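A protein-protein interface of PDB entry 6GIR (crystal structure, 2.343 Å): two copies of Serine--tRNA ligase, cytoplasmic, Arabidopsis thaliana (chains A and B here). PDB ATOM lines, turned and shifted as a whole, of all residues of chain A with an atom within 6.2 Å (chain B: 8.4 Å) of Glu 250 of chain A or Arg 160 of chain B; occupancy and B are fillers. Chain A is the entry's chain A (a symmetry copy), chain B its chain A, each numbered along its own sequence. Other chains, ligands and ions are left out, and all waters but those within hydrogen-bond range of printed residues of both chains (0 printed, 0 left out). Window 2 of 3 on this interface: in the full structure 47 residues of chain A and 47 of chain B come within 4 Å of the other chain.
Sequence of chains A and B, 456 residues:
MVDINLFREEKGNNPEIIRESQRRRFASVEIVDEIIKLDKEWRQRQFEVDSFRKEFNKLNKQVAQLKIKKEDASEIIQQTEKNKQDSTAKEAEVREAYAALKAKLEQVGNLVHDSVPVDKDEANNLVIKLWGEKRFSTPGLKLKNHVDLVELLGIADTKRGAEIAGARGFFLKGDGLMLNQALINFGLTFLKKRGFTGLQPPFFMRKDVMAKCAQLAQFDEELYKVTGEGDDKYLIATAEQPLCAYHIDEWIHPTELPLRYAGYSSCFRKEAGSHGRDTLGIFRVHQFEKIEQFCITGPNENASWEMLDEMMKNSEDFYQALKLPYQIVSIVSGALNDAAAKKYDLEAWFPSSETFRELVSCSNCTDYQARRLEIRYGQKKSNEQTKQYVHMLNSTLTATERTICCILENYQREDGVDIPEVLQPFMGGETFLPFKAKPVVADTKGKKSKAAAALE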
ATOM      1  N   ALA A 245      16.319   5.921   0.492  1.00  0.00           N
ATOM      2  CA  ALA A 245      17.591   6.451  -0.009  1.00  0.00           C
ATOM      3  C   ALA A 245      18.795   5.964   0.771  1.00  0.00           C
ATOM      4  O   ALA A 245      19.853   5.769   0.193  1.00  0.00           O
ATOM      5  CB  ALA A 245      17.579   7.970   0.006  1.00  0.00           C
ATOM      6  N   TYR A 246      18.652   5.841   2.093  1.00  0.00           N
ATOM      7  CA  TYR A 246      19.651   5.168   2.946  1.00  0.00           C
ATOM      8  C   TYR A 246      19.987   3.860   2.235  1.00  0.00           C
ATOM      9  O   TYR A 246      19.052   3.132   1.906  1.00  0.00           O
ATOM     10  CB  TYR A 246      19.026   4.869   4.328  1.00  0.00           C
ATOM     11  CG  TYR A 246      19.987   4.492   5.441  1.00  0.00           C
ATOM     12  CD1 TYR A 246      20.387   3.179   5.636  1.00  0.00           C
ATOM     13  CD2 TYR A 246      20.459   5.451   6.330  1.00  0.00           C
ATOM     14  CE1 TYR A 246      21.254   2.827   6.660  1.00  0.00           C
ATOM     15  CE2 TYR A 246      21.319   5.117   7.362  1.00  0.00           C
ATOM     16  CZ  TYR A 246      21.713   3.806   7.524  1.00  0.00           C
ATOM     17  OH  TYR A 246      22.572   3.493   8.549  1.00  0.00           O
ATOM     18  N   HIS A 247      21.266   3.592   1.944  1.00  0.00           N
ATOM     19  CA  HIS A 247      21.701   2.427   1.098  1.00  0.00           C
ATOM     20  C   HIS A 247      21.641   2.608  -0.432  1.00  0.00           C
ATOM     21  O   HIS A 247      21.779   1.640  -1.182  1.00  0.00           O
ATOM     22  CB  HIS A 247      20.995   1.098   1.425  1.00  0.00           C
ATOM     23  CG  HIS A 247      21.338   0.516   2.753  1.00  0.00           C
ATOM     24  ND1 HIS A 247      22.616   0.132   3.084  1.00  0.00           N
ATOM     25  CD2 HIS A 247      20.557   0.171   3.803  1.00  0.00           C
ATOM     26  CE1 HIS A 247      22.616  -0.395   4.295  1.00  0.00           C
ATOM     27  NE2 HIS A 247      21.379  -0.377   4.756  1.00  0.00           N
ATOM     28  N   ILE A 248      21.420   3.820  -0.906  1.00  0.00           N
ATOM     29  CA  ILE A 248      21.560   4.128  -2.335  1.00  0.00           C
ATOM     30  C   ILE A 248      22.980   3.794  -2.870  1.00  0.00           C
ATOM     31  O   ILE A 248      23.990   3.961  -2.166  1.00  0.00           O
ATOM     32  CB  ILE A 248      21.212   5.603  -2.603  1.00  0.00           C
ATOM     33  CG1 ILE A 248      21.095   5.885  -4.092  1.00  0.00           C
ATOM     34  CG2 ILE A 248      22.221   6.552  -1.946  1.00  0.00           C
ATOM     35  CD1 ILE A 248      20.393   7.202  -4.348  1.00  0.00           C
ATOM     36  N   ASP A 249      23.031   3.274  -4.099  1.00  0.00           N
ATOM     37  CA  ASP A 249      24.273   2.884  -4.756  1.00  0.00           C
ATOM     38  C   ASP A 249      25.103   1.756  -4.111  1.00  0.00           C
ATOM     39  O   ASP A 249      26.086   1.327  -4.712  1.00  0.00           O
ATOM     40  CB  ASP A 249      25.174   4.124  -4.977  1.00  0.00           C
ATOM     41  CG  ASP A 249      25.094   4.678  -6.381  1.00  0.00           C
ATOM     42  OD1 ASP A 249      24.561   4.002  -7.288  1.00  0.00           O
ATOM     43  OD2 ASP A 249      25.592   5.805  -6.578  1.00  0.00           O
ATOM     44  N   GLU A 250      24.721   1.237  -2.947  1.00  0.00           N
ATOM     45  CA  GLU A 250      25.543   0.241  -2.256  1.00  0.00           C
ATOM     46  C   GLU A 250      25.321  -1.186  -2.756  1.00  0.00           C
ATOM     47  O   GLU A 250      24.355  -1.465  -3.455  1.00  0.00           O
ATOM     48  CB  GLU A 250      25.230   0.260  -0.767  1.00  0.00           C
ATOM     49  CG  GLU A 250      25.438   1.605  -0.092  1.00  0.00           C
ATOM     50  CD  GLU A 250      25.267   1.543   1.421  1.00  0.00           C
ATOM     51  OE1 GLU A 250      25.107   2.602   2.041  1.00  0.00           O
ATOM     52  OE2 GLU A 250      25.271   0.451   2.026  1.00  0.00           O
ATOM     53  N   TRP A 251      26.234  -2.082  -2.403  1.00  0.00           N
ATOM     54  CA  TRP A 251      25.944  -3.524  -2.363  1.00  0.00           C
ATOM     55  C   TRP A 251      25.559  -3.916  -0.941  1.00  0.00           C
ATOM     56  O   TRP A 251      25.914  -3.237   0.026  1.00  0.00           O
ATOM     57  CB  TRP A 251      27.139  -4.365  -2.819  1.00  0.00           C
ATOM     58  CG  TRP A 251      27.378  -4.266  -4.286  1.00  0.00           C
ATOM     59  CD1 TRP A 251      27.790  -3.163  -4.979  1.00  0.00           C
ATOM     60  CD2 TRP A 251      27.197  -5.303  -5.251  1.00  0.00           C
ATOM     61  NE1 TRP A 251      27.877  -3.454  -6.316  1.00  0.00           N
ATOM     62  CE2 TRP A 251      27.520  -4.761  -6.511  1.00  0.00           C
ATOM     63  CE3 TRP A 251      26.784  -6.642  -5.170  1.00  0.00           C
ATOM     64  CZ2 TRP A 251      27.462  -5.510  -7.689  1.00  0.00           C
ATOM     65  CZ3 TRP A 251      26.724  -7.394  -6.348  1.00  0.00           C
ATOM     66  CH2 TRP A 251      27.063  -6.819  -7.592  1.00  0.00           C
ATOM     67  N   ILE A 252      24.797  -4.998  -0.827  1.00  0.00           N
ATOM     68  CA  ILE A 252      24.417  -5.568   0.466  1.00  0.00           C
ATOM     69  C   ILE A 252      24.666  -7.059   0.347  1.00  0.00           C
ATOM     70  O   ILE A 252      24.165  -7.701  -0.571  1.00  0.00           O
ATOM     71  CB  ILE A 252      22.960  -5.232   0.847  1.00  0.00           C
ATOM     72  CG1 ILE A 252      22.797  -3.711   0.955  1.00  0.00           C
ATOM     73  CG2 ILE A 252      22.552  -5.894   2.164  1.00  0.00           C
ATOM     74  CD1 ILE A 252      21.415  -3.267   1.394  1.00  0.00           C
ATOM     75  N   GLU A 256      24.140  -9.818   5.375  1.00  0.00           N
ATOM     76  CA  GLU A 256      23.516  -8.640   6.008  1.00  0.00           C
ATOM     77  C   GLU A 256      21.966  -8.727   6.058  1.00  0.00           C
ATOM     78  O   GLU A 256      21.319  -8.009   6.833  1.00  0.00           O
ATOM     79  CB  GLU A 256      23.915  -7.349   5.270  1.00  0.00           C
ATOM     80  CG  GLU A 256      25.406  -7.016   5.188  1.00  0.00           C
ATOM     81  CD  GLU A 256      25.666  -5.690   4.438  1.00  0.00           C
ATOM     82  OE1 GLU A 256      25.108  -4.638   4.843  1.00  0.00           O
ATOM     83  OE2 GLU A 256      26.425  -5.689   3.432  1.00  0.00           O
ATOM     84  N   LEU A 373      17.595   2.904  -7.498  1.00  0.00           N
ATOM     85  CA  LEU A 373      18.624   3.370  -6.556  1.00  0.00           C
ATOM     86  C   LEU A 373      19.944   2.570  -6.608  1.00  0.00           C
ATOM     87  O   LEU A 373      20.863   2.811  -5.807  1.00  0.00           O
ATOM     88  CB  LEU A 373      18.079   3.275  -5.123  1.00  0.00           C
ATOM     89  CG  LEU A 373      16.765   3.945  -4.753  1.00  0.00           C
ATOM     90  CD1 LEU A 373      16.169   3.296  -3.510  1.00  0.00           C
ATOM     91  CD2 LEU A 373      16.985   5.426  -4.545  1.00  0.00           C
ATOM     92  N   GLU A 374      20.040   1.614  -7.523  1.00  0.00           N
ATOM     93  CA  GLU A 374      21.202   0.737  -7.608  1.00  0.00           C
ATOM     94  C   GLU A 374      21.575   0.107  -6.265  1.00  0.00           C
ATOM     95  O   GLU A 374      22.703   0.190  -5.827  1.00  0.00           O
ATOM     96  CB  GLU A 374      22.377   1.464  -8.260  1.00  0.00           C
ATOM     97  CG  GLU A 374      22.083   1.876  -9.690  1.00  0.00           C
ATOM     98  CD  GLU A 374      21.952   0.691 -10.634  1.00  0.00           C
ATOM     99  OE1 GLU A 374      22.055  -0.472 -10.171  1.00  0.00           O
ATOM    100  OE2 GLU A 374      21.764   0.927 -11.854  1.00  0.00           O
ATOM    101  N   ILE A 375      20.587  -0.529  -5.638  1.00  0.00           N
ATOM    102  CA  ILE A 375      20.786  -1.291  -4.423  1.00  0.00           C
ATOM    103  C   ILE A 375      20.889  -2.763  -4.779  1.00  0.00           C
ATOM    104  O   ILE A 375      19.898  -3.459  -4.975  1.00  0.00           O
ATOM    105  CB  ILE A 375      19.714  -1.032  -3.365  1.00  0.00           C
ATOM    106  CG1 ILE A 375      19.497   0.485  -3.241  1.00  0.00           C
ATOM    107  CG2 ILE A 375      20.183  -1.639  -2.041  1.00  0.00           C
ATOM    108  CD1 ILE A 375      18.543   0.955  -2.157  1.00  0.00           C
ATOM    109  N   ARG A 376      22.132  -3.213  -4.819  1.00  0.00           N
ATOM    110  CA  ARG A 376      22.505  -4.450  -5.424  1.00  0.00           C
ATOM    111  C   ARG A 376      22.530  -5.549  -4.405  1.00  0.00           C
ATOM    112  O   ARG A 376      22.587  -5.311  -3.220  1.00  0.00           O
ATOM    113  CB  ARG A 376      23.901  -4.289  -6.020  1.00  0.00           C
ATOM    114  CG  ARG A 376      23.986  -3.294  -7.180  1.00  0.00           C
ATOM    115  CD  ARG A 376      23.152  -3.774  -8.358  1.00  0.00           C
ATOM    116  NE  ARG A 376      23.478  -5.166  -8.663  1.00  0.00           N
ATOM    117  CZ  ARG A 376      24.273  -5.577  -9.646  1.00  0.00           C
ATOM    118  NH1 ARG A 376      24.814  -4.721 -10.503  1.00  0.00           N
ATOM    119  NH2 ARG A 376      24.508  -6.882  -9.791  1.00  0.00           N
ATOM    120  N   TYR A 377      22.517  -6.766  -4.910  1.00  0.00           N
ATOM    121  CA  TYR A 377      22.536  -7.972  -4.119  1.00  0.00           C
ATOM    122  C   TYR A 377      23.503  -8.962  -4.766  1.00  0.00           C
ATOM    123  O   TYR A 377      24.333  -9.538  -4.069  1.00  0.00           O
ATOM    124  CB  TYR A 377      21.118  -8.541  -4.077  1.00  0.00           C
ATOM    125  CG  TYR A 377      21.034  -9.892  -3.462  1.00  0.00           C
ATOM    126  CD1 TYR A 377      20.859 -10.037  -2.103  1.00  0.00           C
ATOM    127  CD2 TYR A 377      21.153 -11.038  -4.241  1.00  0.00           C
ATOM    128  CE1 TYR A 377      20.786 -11.293  -1.525  1.00  0.00           C
ATOM    129  CE2 TYR A 377      21.100 -12.294  -3.670  1.00  0.00           C
ATOM    130  CZ  TYR A 377      20.911 -12.412  -2.315  1.00  0.00           C
ATOM    131  OH  TYR A 377      20.839 -13.648  -1.738  1.00  0.00           O
ATOM    132  N   GLU B 151      30.847   7.704  15.974  1.00  0.00           N
ATOM    133  CA  GLU B 151      31.244   6.743  14.946  1.00  0.00           C
ATOM    134  C   GLU B 151      31.546   5.393  15.579  1.00  0.00           C
ATOM    135  O   GLU B 151      31.054   4.386  15.114  1.00  0.00           O
ATOM    136  CB  GLU B 151      32.450   7.257  14.137  1.00  0.00           C
ATOM    137  CG  GLU B 151      33.054   6.288  13.091  1.00  0.00           C
ATOM    138  CD  GLU B 151      32.155   5.960  11.871  1.00  0.00           C
ATOM    139  OE1 GLU B 151      30.990   6.427  11.775  1.00  0.00           O
ATOM    140  OE2 GLU B 151      32.626   5.216  10.973  1.00  0.00           O
ATOM    141  N   ALA B 156      24.939   7.163  15.076  1.00  0.00           N
ATOM    142  CA  ALA B 156      24.518   8.099  14.055  1.00  0.00           C
ATOM    143  C   ALA B 156      25.056   7.655  12.722  1.00  0.00           C
ATOM    144  O   ALA B 156      26.007   6.897  12.672  1.00  0.00           O
ATOM    145  CB  ALA B 156      25.000   9.500  14.372  1.00  0.00           C
ATOM    146  N   ASP B 157      24.425   8.099  11.645  1.00  0.00           N
ATOM    147  CA  ASP B 157      24.998   7.948  10.318  1.00  0.00           C
ATOM    148  C   ASP B 157      25.090   9.339   9.750  1.00  0.00           C
ATOM    149  O   ASP B 157      24.071   9.950   9.390  1.00  0.00           O
ATOM    150  CB  ASP B 157      24.179   7.024   9.419  1.00  0.00           C
ATOM    151  CG  ASP B 157      25.019   6.434   8.300  1.00  0.00           C
ATOM    152  OD1 ASP B 157      25.813   7.204   7.693  1.00  0.00           O
ATOM    153  OD2 ASP B 157      24.910   5.209   8.037  1.00  0.00           O
ATOM    154  N   THR B 158      26.320   9.857   9.744  1.00  0.00           N
ATOM    155  CA  THR B 158      26.582  11.217   9.311  1.00  0.00           C
ATOM    156  C   THR B 158      26.929  11.284   7.831  1.00  0.00           C
ATOM    157  O   THR B 158      26.520  12.228   7.159  1.00  0.00           O
ATOM    158  CB  THR B 158      27.662  11.918  10.165  1.00  0.00           C
ATOM    159  OG1 THR B 158      28.826  11.093  10.294  1.00  0.00           O
ATOM    160  CG2 THR B 158      27.104  12.235  11.523  1.00  0.00           C
ATOM    161  N   LYS B 159      27.698  10.305   7.349  1.00  0.00           N
ATOM    162  CA  LYS B 159      27.908  10.116   5.924  1.00  0.00           C
ATOM    163  C   LYS B 159      26.568  10.074   5.209  1.00  0.00           C
ATOM    164  O   LYS B 159      26.253  10.982   4.451  1.00  0.00           O
ATOM    165  CB  LYS B 159      28.695   8.841   5.633  1.00  0.00           C
ATOM    166  CG  LYS B 159      30.200   9.030   5.633  1.00  0.00           C
ATOM    167  CD  LYS B 159      30.914   7.739   5.238  1.00  0.00           C
ATOM    168  CE  LYS B 159      32.178   8.002   4.428  1.00  0.00           C
ATOM    169  NZ  LYS B 159      33.178   8.797   5.197  1.00  0.00           N
ATOM    170  N   ARG B 160      25.757   9.060   5.505  1.00  0.00           N
ATOM    171  CA  ARG B 160      24.523   8.836   4.762  1.00  0.00           C
ATOM    172  C   ARG B 160      23.555   9.991   4.852  1.00  0.00           C
ATOM    173  O   ARG B 160      22.998  10.418   3.845  1.00  0.00           O
ATOM    174  CB  ARG B 160      23.841   7.555   5.190  1.00  0.00           C
ATOM    175  CG  ARG B 160      24.604   6.319   4.750  1.00  0.00           C
ATOM    176  CD  ARG B 160      23.740   5.094   4.885  1.00  0.00           C
ATOM    177  NE  ARG B 160      24.366   3.885   4.362  1.00  0.00           N
ATOM    178  CZ  ARG B 160      25.145   3.048   5.045  1.00  0.00           C
ATOM    179  NH1 ARG B 160      25.463   3.279   6.320  1.00  0.00           N
ATOM    180  NH2 ARG B 160      25.607   1.954   4.444  1.00  0.00           N
ATOM    181  N   GLY B 161      23.377  10.512   6.051  1.00  0.00           N
ATOM    182  CA  GLY B 161      22.537  11.691   6.246  1.00  0.00           C
ATOM    183  C   GLY B 161      23.016  12.878   5.444  1.00  0.00           C
ATOM    184  O   GLY B 161      22.207  13.724   5.031  1.00  0.00           O
ATOM    185  N   ALA B 162      24.334  12.961   5.249  1.00  0.00           N
ATOM    186  CA  ALA B 162      24.906  14.044   4.455  1.00  0.00           C
ATOM    187  C   ALA B 162      24.585  13.871   2.973  1.00  0.00           C
ATOM    188  O   ALA B 162      24.249  14.842   2.335  1.00  0.00           O
ATOM    189  CB  ALA B 162      26.405  14.196   4.678  1.00  0.00           C
ATOM    190  N   GLU B 163      24.674  12.644   2.456  1.00  0.00           N
ATOM    191  CA  GLU B 163      24.302  12.331   1.071  1.00  0.00           C
ATOM    192  C   GLU B 163      22.808  12.566   0.797  1.00  0.00           C
ATOM    193  O   GLU B 163      22.430  12.961  -0.309  1.00  0.00           O
ATOM    194  CB  GLU B 163      24.695  10.882   0.681  1.00  0.00           C
ATOM    195  CG  GLU B 163      26.107  10.715   0.099  1.00  0.00           C
ATOM    196  CD  GLU B 163      27.206  10.516   1.146  1.00  0.00           C
ATOM    197  OE1 GLU B 163      27.102   9.550   1.944  1.00  0.00           O
ATOM    198  OE2 GLU B 163      28.190  11.302   1.159  1.00  0.00           O
ATOM    199  N   ILE B 164      21.973  12.334   1.808  1.00  0.00           N
ATOM    200  CA  ILE B 164      20.514  12.474   1.685  1.00  0.00           C
ATOM    201  C   ILE B 164      20.071  13.936   1.919  1.00  0.00           C
ATOM    202  O   ILE B 164      19.274  14.471   1.155  1.00  0.00           O
ATOM    203  CB  ILE B 164      19.766  11.460   2.630  1.00  0.00           C
ATOM    204  CG1 ILE B 164      19.646  10.063   1.992  1.00  0.00           C
ATOM    205  CG2 ILE B 164      18.342  11.916   2.954  1.00  0.00           C
ATOM    206  CD1 ILE B 164      20.925   9.270   1.875  1.00  0.00           C
ATOM    207  N   ALA B 165      20.572  14.570   2.979  1.00  0.00           N
ATOM    208  CA  ALA B 165      20.042  15.861   3.426  1.00  0.00           C
ATOM    209  C   ALA B 165      20.967  17.036   3.207  1.00  0.00           C
ATOM    210  O   ALA B 165      20.620  18.150   3.576  1.00  0.00           O
ATOM    211  CB  ALA B 165      19.663  15.785   4.891  1.00  0.00           C
ATOM    212  N   GLY B 166      22.113  16.808   2.580  1.00  0.00           N
ATOM    213  CA  GLY B 166      23.132  17.835   2.428  1.00  0.00           C
ATOM    214  C   GLY B 166      23.999  17.895   3.670  1.00  0.00           C
ATOM    215  O   GLY B 166      23.942  16.999   4.528  1.00  0.00           O
ATOM    216  N   GLY B 169      23.843  16.746   7.770  1.00  0.00           N
ATOM    217  CA  GLY B 169      22.704  15.865   7.941  1.00  0.00           C
ATOM    218  C   GLY B 169      23.111  14.572   8.609  1.00  0.00           C
ATOM    219  O   GLY B 169      24.231  14.064   8.418  1.00  0.00           O
ATOM    220  N   PHE B 170      22.206  14.035   9.418  1.00  0.00           N
ATOM    221  CA  PHE B 170      22.475  12.775  10.099  1.00  0.00           C
ATOM    222  C   PHE B 170      21.205  12.018  10.414  1.00  0.00           C
ATOM    223  O   PHE B 170      20.127  12.612  10.593  1.00  0.00           O
ATOM    224  CB  PHE B 170      23.256  13.026  11.393  1.00  0.00           C
ATOM    225  CG  PHE B 170      22.463  13.759  12.448  1.00  0.00           C
ATOM    226  CD1 PHE B 170      22.403  15.152  12.452  1.00  0.00           C
ATOM    227  CD2 PHE B 170      21.767  13.052  13.439  1.00  0.00           C
ATOM    228  CE1 PHE B 170      21.667  15.829  13.417  1.00  0.00           C
ATOM    229  CE2 PHE B 170      21.023  13.726  14.389  1.00  0.00           C
ATOM    230  CZ  PHE B 170      20.975  15.116  14.379  1.00  0.00           C
ATOM    231  N   PHE B 171      21.364  10.702  10.493  1.00  0.00           N
ATOM    232  CA  PHE B 171      20.378   9.822  11.091  1.00  0.00           C
ATOM    233  C   PHE B 171      20.763   9.534  12.545  1.00  0.00           C
ATOM    234  O   PHE B 171      21.949   9.439  12.872  1.00  0.00           O
ATOM    235  CB  PHE B 171      20.371   8.485  10.368  1.00  0.00           C
ATOM    236  CG  PHE B 171      19.885   8.550   8.956  1.00  0.00           C
ATOM    237  CD1 PHE B 171      20.714   9.001   7.938  1.00  0.00           C
ATOM    238  CD2 PHE B 171      18.615   8.083   8.623  1.00  0.00           C
ATOM    239  CE1 PHE B 171      20.276   9.013   6.613  1.00  0.00           C
ATOM    240  CE2 PHE B 171      18.168   8.085   7.308  1.00  0.00           C
ATOM    241  CZ  PHE B 171      18.993   8.558   6.301  1.00  0.00           C
ATOM    242  N   LYS B 173      20.547   6.289  14.954  1.00  0.00           N
ATOM    243  CA  LYS B 173      20.500   4.865  14.671  1.00  0.00           C
ATOM    244  C   LYS B 173      20.637   4.078  15.967  1.00  0.00           C
ATOM    245  O   LYS B 173      21.443   4.426  16.834  1.00  0.00           O
ATOM    246  CB  LYS B 173      21.607   4.503  13.676  1.00  0.00           C
ATOM    247  CG  LYS B 173      21.521   3.090  13.129  1.00  0.00           C
ATOM    248  CD  LYS B 173      22.560   2.861  12.043  1.00  0.00           C
ATOM    249  CE  LYS B 173      22.488   1.430  11.511  1.00  0.00           C
ATOM    250  NZ  LYS B 173      22.975   1.288  10.099  1.00  0.00           N
ATOM    251  N   LEU B 280      32.768  14.945  10.858  1.00  0.00           N
ATOM    252  CA  LEU B 280      31.317  14.821  10.729  1.00  0.00           C
ATOM    253  C   LEU B 280      30.701  14.167  11.988  1.00  0.00           C
ATOM    254  O   LEU B 280      30.737  12.935  12.135  1.00  0.00           O
ATOM    255  CB  LEU B 280      30.948  14.020   9.451  1.00  0.00           C
ATOM    256  CG  LEU B 280      30.928  14.687   8.049  1.00  0.00           C
ATOM    257  CD1 LEU B 280      30.710  13.642   6.945  1.00  0.00           C
ATOM    258  CD2 LEU B 280      29.879  15.801   7.937  1.00  0.00           C
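The side-chain carboxylate (OD2) of Asp 157 of chain B sits at hydrogen-bond distance from the side-chain hydroxyl (OH) of Tyr 246 of chain A, at 2.9 Å. The side-chain carboxylate of Glu 250 of chain A lies within salt-bridge range of the guanidinium group of Arg 160 of chain B, at 2.5 Å. NZ of Lys 173 of chain B sits at hydrogen-bond distance from OH of Tyr 246 of chain A, 2.7 Å away.
OD2 of Asp 157 of chain B lies within salt-bridge range of NH1 of Arg 160 of chain B, at 2.6 Å. N of Phe 171 of chain B is in hydrogen-bond range of O of Asp 157 of chain B (3.0 Å). The side-chain carboxylate (OE2) of Glu 250 of chain A is in hydrogen-bond range of a ring nitrogen (ND1) of His 247 of chain A (2.9 Å). N of Arg 376 of chain A is in hydrogen-bond range of O of Glu 250 of chain A, at 3.1 Å.
Among the printed residues, merely in contact across the chains: Ala 245 of chain A with Ile 164 of chain B (3.5 Å), Tyr 246 of chain A with Arg 160 of chain B (3.5 Å), Tyr 246 of chain A with Phe 171 of chain B (3.4 Å) and His 247 of chain A with Arg 160 of chain B (3.8 Å).
Of the printed residues of chain B, Tyr 246 of chain A touches Asp 157, Arg 160, Phe 171 and Lys 173. Printed residues of chain B within 4 Å of His 247 of chain A: Arg 160 (3.8 Å). Glu 256 of chain A touches none of the printed residues of chain B. Ile 375 of chain A touches none of the printed residues of chain B. Of the printed residues of chain A, Ile 164 of chain B touches Ala 245 (3.5 Å).
Printed residues of chain B that touch a printed residue of chain A: Asp 157, Arg 160, Ile 164, Phe 171 and Lys 173. Hydrophobic or aromatic side chains of chain B that line the printed part of chain A: Ile 164 and Phe 171. Along chain B the printed residues that touch a printed residue of chain A span positions 157 to 173. Of the 14 printed residues of chain A, 4 touch a printed residue of chain B. Hydrophobic or aromatic side chains of chain A within 4 Å of the printed part of chain B: Ala 245, Tyr 246 and His 247.
No position is printed for both chains. Of the 7 pairs that touch across the chains among the printed residues, none has its exchanged pair printed and touching as well.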
